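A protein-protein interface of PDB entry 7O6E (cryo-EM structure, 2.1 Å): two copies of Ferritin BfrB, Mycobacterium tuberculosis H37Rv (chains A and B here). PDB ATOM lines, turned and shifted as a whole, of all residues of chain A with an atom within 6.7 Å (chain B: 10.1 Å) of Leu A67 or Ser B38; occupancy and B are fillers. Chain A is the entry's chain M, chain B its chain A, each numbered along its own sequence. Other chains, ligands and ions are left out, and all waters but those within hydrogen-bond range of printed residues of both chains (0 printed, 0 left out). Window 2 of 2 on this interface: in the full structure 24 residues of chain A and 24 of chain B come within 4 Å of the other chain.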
ATOM      1  N   MET A  60     -17.679 -31.350  -1.721  1.00  0.00           N
ATOM      2  CA  MET A  60     -18.941 -31.015  -2.340  1.00  0.00           C
ATOM      3  C   MET A  60     -19.431 -29.629  -1.943  1.00  0.00           C
ATOM      4  O   MET A  60     -20.056 -28.945  -2.744  1.00  0.00           O
ATOM      5  CB  MET A  60     -19.973 -32.053  -1.981  1.00  0.00           C
ATOM      6  CG  MET A  60     -19.717 -33.351  -2.624  1.00  0.00           C
ATOM      7  SD  MET A  60     -18.845 -33.289  -4.187  1.00  0.00           S
ATOM      8  CE  MET A  60     -20.228 -33.390  -5.298  1.00  0.00           C
ATOM      9  N   LEU A  62     -17.489 -27.021  -1.295  1.00  0.00           N
ATOM     10  CA  LEU A  62     -16.717 -26.091  -2.103  1.00  0.00           C
ATOM     11  C   LEU A  62     -17.230 -26.065  -3.536  1.00  0.00           C
ATOM     12  O   LEU A  62     -17.351 -24.996  -4.147  1.00  0.00           O
ATOM     13  CB  LEU A  62     -15.242 -26.460  -2.058  1.00  0.00           C
ATOM     14  CG  LEU A  62     -14.602 -26.508  -0.676  1.00  0.00           C
ATOM     15  CD1 LEU A  62     -13.173 -26.910  -0.732  1.00  0.00           C
ATOM     16  CD2 LEU A  62     -14.669 -25.215   0.006  1.00  0.00           C
ATOM     17  N   VAL A  63     -17.554 -27.231  -4.073  1.00  0.00           N
ATOM     18  CA  VAL A  63     -18.168 -27.305  -5.388  1.00  0.00           C
ATOM     19  C   VAL A  63     -19.451 -26.487  -5.415  1.00  0.00           C
ATOM     20  O   VAL A  63     -19.661 -25.666  -6.305  1.00  0.00           O
ATOM     21  CB  VAL A  63     -18.435 -28.770  -5.773  1.00  0.00           C
ATOM     22  CG1 VAL A  63     -19.398 -28.833  -6.920  1.00  0.00           C
ATOM     23  CG2 VAL A  63     -17.172 -29.456  -6.105  1.00  0.00           C
ATOM     24  N   GLN A  64     -20.322 -26.709  -4.442  1.00  0.00           N
ATOM     25  CA  GLN A  64     -21.616 -26.047  -4.417  1.00  0.00           C
ATOM     26  C   GLN A  64     -21.455 -24.542  -4.329  1.00  0.00           C
ATOM     27  O   GLN A  64     -22.217 -23.789  -4.925  1.00  0.00           O
ATOM     28  CB  GLN A  64     -22.438 -26.534  -3.236  1.00  0.00           C
ATOM     29  CG  GLN A  64     -23.796 -25.829  -3.108  1.00  0.00           C
ATOM     30  CD  GLN A  64     -24.696 -26.176  -4.264  1.00  0.00           C
ATOM     31  OE1 GLN A  64     -24.906 -27.336  -4.545  1.00  0.00           O
ATOM     32  NE2 GLN A  64     -25.190 -25.191  -4.949  1.00  0.00           N
ATOM     33  N   HIS A  65     -20.492 -24.096  -3.553  1.00  0.00           N
ATOM     34  CA  HIS A  65     -20.208 -22.686  -3.480  1.00  0.00           C
ATOM     35  C   HIS A  65     -19.816 -22.134  -4.836  1.00  0.00           C
ATOM     36  O   HIS A  65     -20.235 -21.040  -5.204  1.00  0.00           O
ATOM     37  CB  HIS A  65     -19.109 -22.418  -2.471  1.00  0.00           C
ATOM     38  CG  HIS A  65     -18.819 -20.976  -2.290  1.00  0.00           C
ATOM     39  ND1 HIS A  65     -19.607 -20.158  -1.513  1.00  0.00           N
ATOM     40  CD2 HIS A  65     -17.848 -20.190  -2.800  1.00  0.00           C
ATOM     41  CE1 HIS A  65     -19.131 -18.933  -1.547  1.00  0.00           C
ATOM     42  NE2 HIS A  65     -18.059 -18.927  -2.312  1.00  0.00           N
ATOM     43  N   LEU A  66     -18.999 -22.852  -5.581  1.00  0.00           N
ATOM     44  CA  LEU A  66     -18.688 -22.340  -6.897  1.00  0.00           C
ATOM     45  C   LEU A  66     -19.904 -22.374  -7.820  1.00  0.00           C
ATOM     46  O   LEU A  66     -20.069 -21.484  -8.642  1.00  0.00           O
ATOM     47  CB  LEU A  66     -17.514 -23.093  -7.495  1.00  0.00           C
ATOM     48  CG  LEU A  66     -16.144 -22.866  -6.854  1.00  0.00           C
ATOM     49  CD1 LEU A  66     -15.066 -23.621  -7.604  1.00  0.00           C
ATOM     50  CD2 LEU A  66     -15.766 -21.401  -6.742  1.00  0.00           C
ATOM     51  N   LEU A  67     -20.766 -23.373  -7.692  1.00  0.00           N
ATOM     52  CA  LEU A  67     -21.989 -23.396  -8.483  1.00  0.00           C
ATOM     53  C   LEU A  67     -22.894 -22.218  -8.161  1.00  0.00           C
ATOM     54  O   LEU A  67     -23.472 -21.620  -9.060  1.00  0.00           O
ATOM     55  CB  LEU A  67     -22.748 -24.681  -8.248  1.00  0.00           C
ATOM     56  CG  LEU A  67     -22.067 -25.881  -8.817  1.00  0.00           C
ATOM     57  CD1 LEU A  67     -22.723 -27.061  -8.173  1.00  0.00           C
ATOM     58  CD2 LEU A  67     -22.175 -25.906 -10.340  1.00  0.00           C
ATOM     59  N   ASP A  68     -23.016 -21.877  -6.887  1.00  0.00           N
ATOM     60  CA  ASP A  68     -23.927 -20.832  -6.465  1.00  0.00           C
ATOM     61  C   ASP A  68     -23.483 -19.463  -6.942  1.00  0.00           C
ATOM     62  O   ASP A  68     -24.316 -18.590  -7.144  1.00  0.00           O
ATOM     63  CB  ASP A  68     -24.054 -20.808  -4.954  1.00  0.00           C
ATOM     64  CG  ASP A  68     -24.700 -22.037  -4.411  1.00  0.00           C
ATOM     65  OD1 ASP A  68     -25.562 -22.620  -5.077  1.00  0.00           O
ATOM     66  OD2 ASP A  68     -24.380 -22.420  -3.291  1.00  0.00           O
ATOM     67  N   ARG A  69     -22.196 -19.259  -7.115  1.00  0.00           N
ATOM     68  CA  ARG A  69     -21.675 -17.999  -7.587  1.00  0.00           C
ATOM     69  C   ARG A  69     -21.474 -18.010  -9.080  1.00  0.00           C
ATOM     70  O   ARG A  69     -20.901 -17.074  -9.617  1.00  0.00           O
ATOM     71  CB  ARG A  69     -20.389 -17.688  -6.850  1.00  0.00           C
ATOM     72  CG  ARG A  69     -20.678 -17.586  -5.385  1.00  0.00           C
ATOM     73  CD  ARG A  69     -19.545 -17.140  -4.565  1.00  0.00           C
ATOM     74  NE  ARG A  69     -19.015 -15.878  -5.016  1.00  0.00           N
ATOM     75  CZ  ARG A  69     -17.868 -15.373  -4.612  1.00  0.00           C
ATOM     76  NH1 ARG A  69     -17.133 -16.028  -3.729  1.00  0.00           N
ATOM     77  NH2 ARG A  69     -17.456 -14.236  -5.111  1.00  0.00           N
ATOM     78  N   ASP A  70     -21.935 -19.058  -9.741  1.00  0.00           N
ATOM     79  CA  ASP A  70     -21.813 -19.236 -11.174  1.00  0.00           C
ATOM     80  C   ASP A  70     -20.368 -19.099 -11.622  1.00  0.00           C
ATOM     81  O   ASP A  70     -20.069 -18.477 -12.628  1.00  0.00           O
ATOM     82  CB  ASP A  70     -22.710 -18.264 -11.929  1.00  0.00           C
ATOM     83  CG  ASP A  70     -24.144 -18.725 -11.982  1.00  0.00           C
ATOM     84  OD1 ASP A  70     -24.676 -19.181 -10.945  1.00  0.00           O
ATOM     85  OD2 ASP A  70     -24.758 -18.629 -13.066  1.00  0.00           O
ATOM     86  N   LEU A  71     -19.469 -19.638 -10.838  1.00  0.00           N
ATOM     87  CA  LEU A  71     -18.071 -19.661 -11.197  1.00  0.00           C
ATOM     88  C   LEU A  71     -17.759 -21.028 -11.761  1.00  0.00           C
ATOM     89  O   LEU A  71     -18.348 -22.027 -11.359  1.00  0.00           O
ATOM     90  CB  LEU A  71     -17.168 -19.339 -10.011  1.00  0.00           C
ATOM     91  CG  LEU A  71     -17.261 -17.929  -9.446  1.00  0.00           C
ATOM     92  CD1 LEU A  71     -16.274 -17.747  -8.313  1.00  0.00           C
ATOM     93  CD2 LEU A  71     -17.072 -16.873 -10.485  1.00  0.00           C
ATOM     94  N   VAL A  73     -16.350 -24.442 -12.302  1.00  0.00           N
ATOM     95  CA  VAL A  73     -15.801 -25.448 -11.408  1.00  0.00           C
ATOM     96  C   VAL A  73     -15.594 -26.738 -12.184  1.00  0.00           C
ATOM     97  O   VAL A  73     -16.474 -27.150 -12.932  1.00  0.00           O
ATOM     98  CB  VAL A  73     -16.710 -25.680 -10.181  1.00  0.00           C
ATOM     99  CG1 VAL A  73     -18.129 -25.884 -10.572  1.00  0.00           C
ATOM    100  CG2 VAL A  73     -16.224 -26.848  -9.380  1.00  0.00           C
ATOM    101  N   ALA A 177     -23.160 -29.941  -2.752  1.00  0.00           N
ATOM    102  CA  ALA A 177     -23.678 -30.352  -4.049  1.00  0.00           C
ATOM    103  C   ALA A 177     -23.986 -31.839  -4.026  1.00  0.00           C
ATOM    104  O   ALA A 177     -23.134 -32.655  -3.680  1.00  0.00           O
ATOM    105  CB  ALA A 177     -22.686 -30.023  -5.156  1.00  0.00           C
ATOM    106  N   VAL B  30     -19.637 -37.805 -10.843  1.00  0.00           N
ATOM    107  CA  VAL B  30     -19.712 -36.539 -10.128  1.00  0.00           C
ATOM    108  C   VAL B  30     -19.542 -35.367 -11.088  1.00  0.00           C
ATOM    109  O   VAL B  30     -20.262 -34.371 -11.013  1.00  0.00           O
ATOM    110  CB  VAL B  30     -18.649 -36.489  -9.014  1.00  0.00           C
ATOM    111  CG1 VAL B  30     -18.524 -35.099  -8.471  1.00  0.00           C
ATOM    112  CG2 VAL B  30     -18.970 -37.425  -7.924  1.00  0.00           C
ATOM    113  N   ALA B  31     -18.557 -35.449 -11.972  1.00  0.00           N
ATOM    114  CA  ALA B  31     -18.340 -34.360 -12.915  1.00  0.00           C
ATOM    115  C   ALA B  31     -19.569 -34.140 -13.781  1.00  0.00           C
ATOM    116  O   ALA B  31     -19.970 -33.004 -14.035  1.00  0.00           O
ATOM    117  CB  ALA B  31     -17.125 -34.638 -13.784  1.00  0.00           C
ATOM    118  N   ILE B  32     -20.199 -35.220 -14.201  1.00  0.00           N
ATOM    119  CA  ILE B  32     -21.389 -35.110 -15.017  1.00  0.00           C
ATOM    120  C   ILE B  32     -22.523 -34.482 -14.227  1.00  0.00           C
ATOM    121  O   ILE B  32     -23.236 -33.618 -14.729  1.00  0.00           O
ATOM    122  CB  ILE B  32     -21.767 -36.486 -15.577  1.00  0.00           C
ATOM    123  CG1 ILE B  32     -20.880 -36.810 -16.767  1.00  0.00           C
ATOM    124  CG2 ILE B  32     -23.205 -36.539 -15.960  1.00  0.00           C
ATOM    125  CD1 ILE B  32     -21.053 -38.167 -17.206  1.00  0.00           C
ATOM    126  N   ALA B  33     -22.702 -34.894 -12.982  1.00  0.00           N
ATOM    127  CA  ALA B  33     -23.764 -34.306 -12.179  1.00  0.00           C
ATOM    128  C   ALA B  33     -23.543 -32.814 -11.962  1.00  0.00           C
ATOM    129  O   ALA B  33     -24.475 -32.021 -12.072  1.00  0.00           O
ATOM    130  CB  ALA B  33     -23.883 -35.026 -10.847  1.00  0.00           C
ATOM    131  N   VAL B  34     -22.324 -32.418 -11.677  1.00  0.00           N
ATOM    132  CA  VAL B  34     -22.035 -31.026 -11.477  1.00  0.00           C
ATOM    133  C   VAL B  34     -22.323 -30.265 -12.766  1.00  0.00           C
ATOM    134  O   VAL B  34     -22.870 -29.178 -12.728  1.00  0.00           O
ATOM    135  CB  VAL B  34     -20.604 -30.836 -10.915  1.00  0.00           C
ATOM    136  CG1 VAL B  34     -20.182 -29.375 -10.932  1.00  0.00           C
ATOM    137  CG2 VAL B  34     -20.529 -31.389  -9.505  1.00  0.00           C
ATOM    138  N   TYR B  35     -21.986 -30.839 -13.905  1.00  0.00           N
ATOM    139  CA  TYR B  35     -22.296 -30.222 -15.176  1.00  0.00           C
ATOM    140  C   TYR B  35     -23.795 -30.029 -15.337  1.00  0.00           C
ATOM    141  O   TYR B  35     -24.246 -28.973 -15.765  1.00  0.00           O
ATOM    142  CB  TYR B  35     -21.763 -31.066 -16.314  1.00  0.00           C
ATOM    143  CG  TYR B  35     -22.346 -30.652 -17.607  1.00  0.00           C
ATOM    144  CD1 TYR B  35     -21.973 -29.467 -18.210  1.00  0.00           C
ATOM    145  CD2 TYR B  35     -23.340 -31.398 -18.187  1.00  0.00           C
ATOM    146  CE1 TYR B  35     -22.518 -29.063 -19.386  1.00  0.00           C
ATOM    147  CE2 TYR B  35     -23.911 -31.001 -19.345  1.00  0.00           C
ATOM    148  CZ  TYR B  35     -23.484 -29.837 -19.956  1.00  0.00           C
ATOM    149  OH  TYR B  35     -24.072 -29.440 -21.102  1.00  0.00           O
ATOM    150  N   PHE B  36     -24.574 -31.059 -15.045  1.00  0.00           N
ATOM    151  CA  PHE B  36     -26.015 -30.911 -15.096  1.00  0.00           C
ATOM    152  C   PHE B  36     -26.484 -29.873 -14.099  1.00  0.00           C
ATOM    153  O   PHE B  36     -27.315 -29.030 -14.419  1.00  0.00           O
ATOM    154  CB  PHE B  36     -26.724 -32.237 -14.838  1.00  0.00           C
ATOM    155  CG  PHE B  36     -26.722 -33.145 -16.009  1.00  0.00           C
ATOM    156  CD1 PHE B  36     -26.791 -32.641 -17.293  1.00  0.00           C
ATOM    157  CD2 PHE B  36     -26.631 -34.503 -15.840  1.00  0.00           C
ATOM    158  CE1 PHE B  36     -26.772 -33.474 -18.372  1.00  0.00           C
ATOM    159  CE2 PHE B  36     -26.618 -35.345 -16.915  1.00  0.00           C
ATOM    160  CZ  PHE B  36     -26.680 -34.836 -18.182  1.00  0.00           C
ATOM    161  N   ASP B  37     -25.973 -29.901 -12.885  1.00  0.00           N
ATOM    162  CA  ASP B  37     -26.341 -28.935 -11.866  1.00  0.00           C
ATOM    163  C   ASP B  37     -26.154 -27.512 -12.348  1.00  0.00           C
ATOM    164  O   ASP B  37     -26.997 -26.672 -12.116  1.00  0.00           O
ATOM    165  CB  ASP B  37     -25.507 -29.144 -10.606  1.00  0.00           C
ATOM    166  CG  ASP B  37     -26.271 -28.871  -9.350  1.00  0.00           C
ATOM    167  OD1 ASP B  37     -26.644 -27.708  -9.115  1.00  0.00           O
ATOM    168  OD2 ASP B  37     -26.497 -29.822  -8.584  1.00  0.00           O
ATOM    169  N   SER B  38     -25.077 -27.252 -13.049  1.00  0.00           N
ATOM    170  CA  SER B  38     -24.769 -25.919 -13.523  1.00  0.00           C
ATOM    171  C   SER B  38     -25.436 -25.573 -14.845  1.00  0.00           C
ATOM    172  O   SER B  38     -25.210 -24.490 -15.358  1.00  0.00           O
ATOM    173  CB  SER B  38     -23.275 -25.751 -13.683  1.00  0.00           C
ATOM    174  OG  SER B  38     -22.802 -26.437 -14.806  1.00  0.00           O
ATOM    175  N   GLU B  39     -26.192 -26.484 -15.429  1.00  0.00           N
ATOM    176  CA  GLU B  39     -27.063 -26.195 -16.549  1.00  0.00           C
ATOM    177  C   GLU B  39     -28.509 -26.107 -16.110  1.00  0.00           C
ATOM    178  O   GLU B  39     -29.396 -26.104 -16.948  1.00  0.00           O
ATOM    179  CB  GLU B  39     -26.944 -27.269 -17.619  1.00  0.00           C
ATOM    180  CG  GLU B  39     -25.605 -27.413 -18.250  1.00  0.00           C
ATOM    181  CD  GLU B  39     -25.226 -26.205 -19.018  1.00  0.00           C
ATOM    182  OE1 GLU B  39     -24.035 -25.970 -19.202  1.00  0.00           O
ATOM    183  OE2 GLU B  39     -26.115 -25.456 -19.431  1.00  0.00           O
ATOM    184  N   ASP B  40     -28.757 -26.140 -14.816  1.00  0.00           N
ATOM    185  CA  ASP B  40     -30.100 -26.107 -14.256  1.00  0.00           C
ATOM    186  C   ASP B  40     -30.954 -27.284 -14.719  1.00  0.00           C
ATOM    187  O   ASP B  40     -32.105 -27.119 -15.092  1.00  0.00           O
ATOM    188  CB  ASP B  40     -30.784 -24.777 -14.571  1.00  0.00           C
ATOM    189  CG  ASP B  40     -29.929 -23.607 -14.208  1.00  0.00           C
ATOM    190  OD1 ASP B  40     -29.768 -23.384 -13.014  1.00  0.00           O
ATOM    191  OD2 ASP B  40     -29.387 -22.943 -15.103  1.00  0.00           O
ATOM    192  N   LEU B  41     -30.391 -28.455 -14.709  1.00  0.00           N
ATOM    193  CA  LEU B  41     -31.145 -29.678 -14.881  1.00  0.00           C
ATOM    194  C   LEU B  41     -31.117 -30.457 -13.579  1.00  0.00           C
ATOM    195  O   LEU B  41     -30.491 -31.515 -13.495  1.00  0.00           O
ATOM    196  CB  LEU B  41     -30.576 -30.469 -16.046  1.00  0.00           C
ATOM    197  CG  LEU B  41     -30.456 -29.553 -17.255  1.00  0.00           C
ATOM    198  CD1 LEU B  41     -29.485 -30.031 -18.309  1.00  0.00           C
ATOM    199  CD2 LEU B  41     -31.845 -29.375 -17.842  1.00  0.00           C
ATOM    200  N   PRO B  42     -31.789 -29.970 -12.500  1.00  0.00           N
ATOM    201  CA  PRO B  42     -31.695 -30.603 -11.186  1.00  0.00           C
ATOM    202  C   PRO B  42     -32.064 -32.087 -11.190  1.00  0.00           C
ATOM    203  O   PRO B  42     -31.455 -32.821 -10.453  1.00  0.00           O
ATOM    204  CB  PRO B  42     -32.712 -29.863 -10.305  1.00  0.00           C
ATOM    205  CG  PRO B  42     -33.660 -29.232 -11.278  1.00  0.00           C
ATOM    206  CD  PRO B  42     -32.749 -28.840 -12.414  1.00  0.00           C
ATOM    207  N   GLN B  43     -33.049 -32.486 -11.985  1.00  0.00           N
ATOM    208  CA  GLN B  43     -33.437 -33.882 -11.933  1.00  0.00           C
ATOM    209  C   GLN B  43     -32.315 -34.773 -12.446  1.00  0.00           C
ATOM    210  O   GLN B  43     -31.965 -35.772 -11.813  1.00  0.00           O
ATOM    211  CB  GLN B  43     -34.719 -34.094 -12.729  1.00  0.00           C
ATOM    212  CG  GLN B  43     -35.855 -33.232 -12.293  1.00  0.00           C
ATOM    213  CD  GLN B  43     -36.280 -33.510 -10.888  1.00  0.00           C
ATOM    214  OE1 GLN B  43     -36.386 -34.647 -10.469  1.00  0.00           O
ATOM    215  NE2 GLN B  43     -36.486 -32.470 -10.144  1.00  0.00           N
ATOM    216  N   LEU B  44     -31.697 -34.384 -13.551  1.00  0.00           N
ATOM    217  CA  LEU B  44     -30.548 -35.116 -14.046  1.00  0.00           C
ATOM    218  C   LEU B  44     -29.395 -35.062 -13.068  1.00  0.00           C
ATOM    219  O   LEU B  44     -28.711 -36.062 -12.856  1.00  0.00           O
ATOM    220  CB  LEU B  44     -30.107 -34.559 -15.382  1.00  0.00           C
ATOM    221  CG  LEU B  44     -30.996 -34.952 -16.543  1.00  0.00           C
ATOM    222  CD1 LEU B  44     -30.494 -34.265 -17.775  1.00  0.00           C
ATOM    223  CD2 LEU B  44     -31.023 -36.460 -16.695  1.00  0.00           C
ATOM    224  N   ALA B  45     -29.153 -33.898 -12.486  1.00  0.00           N
ATOM    225  CA  ALA B  45     -28.048 -33.772 -11.557  1.00  0.00           C
ATOM    226  C   ALA B  45     -28.258 -34.673 -10.352  1.00  0.00           C
ATOM    227  O   ALA B  45     -27.341 -35.368  -9.925  1.00  0.00           O
ATOM    228  CB  ALA B  45     -27.860 -32.320 -11.138  1.00  0.00           C
ATOM    229  N   LYS B  46     -29.477 -34.682  -9.822  1.00  0.00           N
ATOM    230  CA  LYS B  46     -29.791 -35.545  -8.659  1.00  0.00           C
ATOM    231  C   LYS B  46     -29.541 -37.011  -9.047  1.00  0.00           C
ATOM    232  O   LYS B  46     -28.922 -37.724  -8.251  1.00  0.00           O
ATOM    233  CB  LYS B  46     -31.233 -35.331  -8.198  1.00  0.00           C
ATOM    234  CG  LYS B  46     -31.734 -36.326  -7.164  1.00  0.00           C
ATOM    235  CD  LYS B  46     -32.732 -35.720  -6.208  1.00  0.00           C
ATOM    236  CE  LYS B  46     -34.117 -35.628  -6.806  1.00  0.00           C
ATOM    237  NZ  LYS B  46     -34.715 -36.972  -6.968  1.00  0.00           N
ATOM    238  N   TYR B  49     -25.728 -37.593  -9.149  1.00  0.00           N
ATOM    239  CA  TYR B  49     -25.141 -37.644  -7.813  1.00  0.00           C
ATOM    240  C   TYR B  49     -25.367 -39.007  -7.175  1.00  0.00           C
ATOM    241  O   TYR B  49     -24.446 -39.601  -6.603  1.00  0.00           O
ATOM    242  CB  TYR B  49     -25.728 -36.563  -6.921  1.00  0.00           C
ATOM    243  CG  TYR B  49     -25.243 -35.197  -7.219  1.00  0.00           C
ATOM    244  CD1 TYR B  49     -23.892 -34.911  -7.241  1.00  0.00           C
ATOM    245  CD2 TYR B  49     -26.132 -34.191  -7.484  1.00  0.00           C
ATOM    246  CE1 TYR B  49     -23.447 -33.659  -7.513  1.00  0.00           C
ATOM    247  CE2 TYR B  49     -25.713 -32.949  -7.756  1.00  0.00           C
ATOM    248  CZ  TYR B  49     -24.369 -32.674  -7.770  1.00  0.00           C
ATOM    249  OH  TYR B  49     -23.979 -31.428  -8.057  1.00  0.00           O
ATOM    250  N   ASN B  83     -15.059 -32.645 -17.943  1.00  0.00           N
ATOM    251  CA  ASN B  83     -15.995 -31.678 -17.360  1.00  0.00           C
ATOM    252  C   ASN B  83     -16.715 -30.871 -18.451  1.00  0.00           C
ATOM    253  O   ASN B  83     -17.842 -30.488 -18.276  1.00  0.00           O
ATOM    254  CB  ASN B  83     -15.241 -30.731 -16.427  1.00  0.00           C
ATOM    255  CG  ASN B  83     -14.755 -31.418 -15.165  1.00  0.00           C
ATOM    256  OD1 ASN B  83     -15.504 -31.585 -14.211  1.00  0.00           O
ATOM    257  ND2 ASN B  83     -13.493 -31.814 -15.155  1.00  0.00           N
ATOM    258  N   GLN B  84     -16.065 -30.608 -19.568  1.00  0.00           N
ATOM    259  CA  GLN B  84     -16.660 -29.883 -20.684  1.00  0.00           C
ATOM    260  C   GLN B  84     -17.653 -30.732 -21.442  1.00  0.00           C
ATOM    261  O   GLN B  84     -17.330 -31.827 -21.884  1.00  0.00           O
ATOM    262  CB  GLN B  84     -15.583 -29.426 -21.647  1.00  0.00           C
ATOM    263  CG  GLN B  84     -14.629 -28.483 -21.068  1.00  0.00           C
ATOM    264  CD  GLN B  84     -15.310 -27.309 -20.458  1.00  0.00           C
ATOM    265  OE1 GLN B  84     -15.964 -27.421 -19.432  1.00  0.00           O
ATOM    266  NE2 GLN B  84     -15.158 -26.160 -21.086  1.00  0.00           N
ATOM    267  N   PHE B  85     -18.831 -30.208 -21.651  1.00  0.00           N
ATOM    268  CA  PHE B  85     -19.748 -30.836 -22.570  1.00  0.00           C
ATOM    269  C   PHE B  85     -20.429 -29.762 -23.384  1.00  0.00           C
ATOM    270  O   PHE B  85     -20.799 -28.733 -22.839  1.00  0.00           O
ATOM    271  CB  PHE B  85     -20.762 -31.671 -21.805  1.00  0.00           C
ATOM    272  CG  PHE B  85     -20.149 -32.773 -20.987  1.00  0.00           C
ATOM    273  CD1 PHE B  85     -19.857 -33.993 -21.550  1.00  0.00           C
ATOM    274  CD2 PHE B  85     -19.878 -32.587 -19.644  1.00  0.00           C
ATOM    275  CE1 PHE B  85     -19.313 -35.012 -20.794  1.00  0.00           C
ATOM    276  CE2 PHE B  85     -19.318 -33.590 -18.883  1.00  0.00           C
ATOM    277  CZ  PHE B  85     -19.035 -34.811 -19.453  1.00  0.00           C
ATOM    278  N   PRO B  88     -26.232 -31.386 -23.044  1.00  0.00           N
ATOM    279  CA  PRO B  88     -26.501 -32.499 -22.126  1.00  0.00           C
ATOM    280  C   PRO B  88     -26.486 -33.875 -22.755  1.00  0.00           C
ATOM    281  O   PRO B  88     -26.113 -34.853 -22.092  1.00  0.00           O
ATOM    282  CB  PRO B  88     -27.885 -32.152 -21.580  1.00  0.00           C
ATOM    283  CG  PRO B  88     -28.010 -30.737 -21.785  1.00  0.00           C
ATOM    284  CD  PRO B  88     -27.220 -30.313 -22.917  1.00  0.00           C
ATOM    285  N   LEU B 153     -35.090 -29.433 -23.324  1.00  0.00           N
ATOM    286  CA  LEU B 153     -34.578 -30.097 -22.133  1.00  0.00           C
ATOM    287  C   LEU B 153     -35.608 -30.274 -21.030  1.00  0.00           C
ATOM    288  O   LEU B 153     -35.446 -31.168 -20.196  1.00  0.00           O
ATOM    289  CB  LEU B 153     -33.395 -29.323 -21.614  1.00  0.00           C
ATOM    290  CG  LEU B 153     -32.304 -29.304 -22.648  1.00  0.00           C
ATOM    291  CD1 LEU B 153     -31.244 -28.332 -22.241  1.00  0.00           C
ATOM    292  CD2 LEU B 153     -31.737 -30.701 -22.832  1.00  0.00           C
ATOM    293  N   GLU B 157     -36.105 -33.519 -18.384  1.00  0.00           N
ATOM    294  CA  GLU B 157     -36.215 -33.421 -16.938  1.00  0.00           C
ATOM    295  C   GLU B 157     -37.513 -34.021 -16.413  1.00  0.00           C
ATOM    296  O   GLU B 157     -37.516 -34.674 -15.370  1.00  0.00           O
ATOM    297  CB  GLU B 157     -36.080 -31.973 -16.506  1.00  0.00           C
ATOM    298  CG  GLU B 157     -34.652 -31.496 -16.491  1.00  0.00           C
ATOM    299  CD  GLU B 157     -33.962 -31.752 -15.154  1.00  0.00           C
ATOM    300  OE1 GLU B 157     -33.100 -32.646 -15.105  1.00  0.00           O
ATOM    301  OE2 GLU B 157     -34.279 -31.075 -14.160  1.00  0.00           O
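The side-chain hydroxyl (OG) of Ser B38 lies within hydrogen-bond range of the backbone carbonyl oxygen (O) of Val B34 (3.4 Å). The backbone carbonyl oxygen of Tyr B35 is in hydrogen-bond range of the side-chain hydroxyl of Ser B38 (3.1 Å). The side-chain hydroxyl (OH) of Tyr B49 sits at hydrogen-bond distance from the side-chain carboxylate (OD2) of Asp B37. The backbone carbonyl oxygen (O) of Met A60 lies within hydrogen-bond range of the backbone NH (N) of Ala A177 (3.3 Å).
Met A60 touches Val B30 (CE to CG1, 3.99 Å). Met A60 touches Tyr B49 (CE to CE1, 3.9 Å). Val B34 touches Val A63. Ser B38 touches Leu A67 (CB to CD2, 3.5 Å). Ala A177 touches Tyr B49 (CB to OH, 3.5 Å).
Leu A67 touches just one residue of chain B: Ser B38 (3.5 Å). Ser B38 touches just one residue of chain A: Leu A67 (3.5 Å). No residue of chain B comes within 4 Å of Gln A64. No residue of chain B comes within 4 Å of Leu A66. No residue of chain B comes within 4 Å of Asp A68. No residue of chain B comes within 4 Å of Asp A70. Printed residues of chain B within 4 Å of Ala A177: Tyr B49. Printed residues of chain A within 4 Å of Val B34: Val A63. Of the printed residues of chain A, Tyr B49 touches Met A60 and Ala A177. Printed residues of chain B within 4 Å of Val A63: Val B34. Printed residues of chain B within 4 Å of Met A60: Val B30 and Tyr B49. Gln B43 touches none of the printed residues of chain A. Asn B83 touches none of the printed residues of chain A. The nearest residue of chain B that does not touch Leu A67 is Val B34 (4.04 Å).
Of the 24 printed residues of chain B, 4 touch a printed residue of chain A. Among the printed residues, no Asp or Glu carboxylate lies within 4 Å of a Lys or Arg side-chain nitrogen of the other chain.
No position is printed for both chains.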
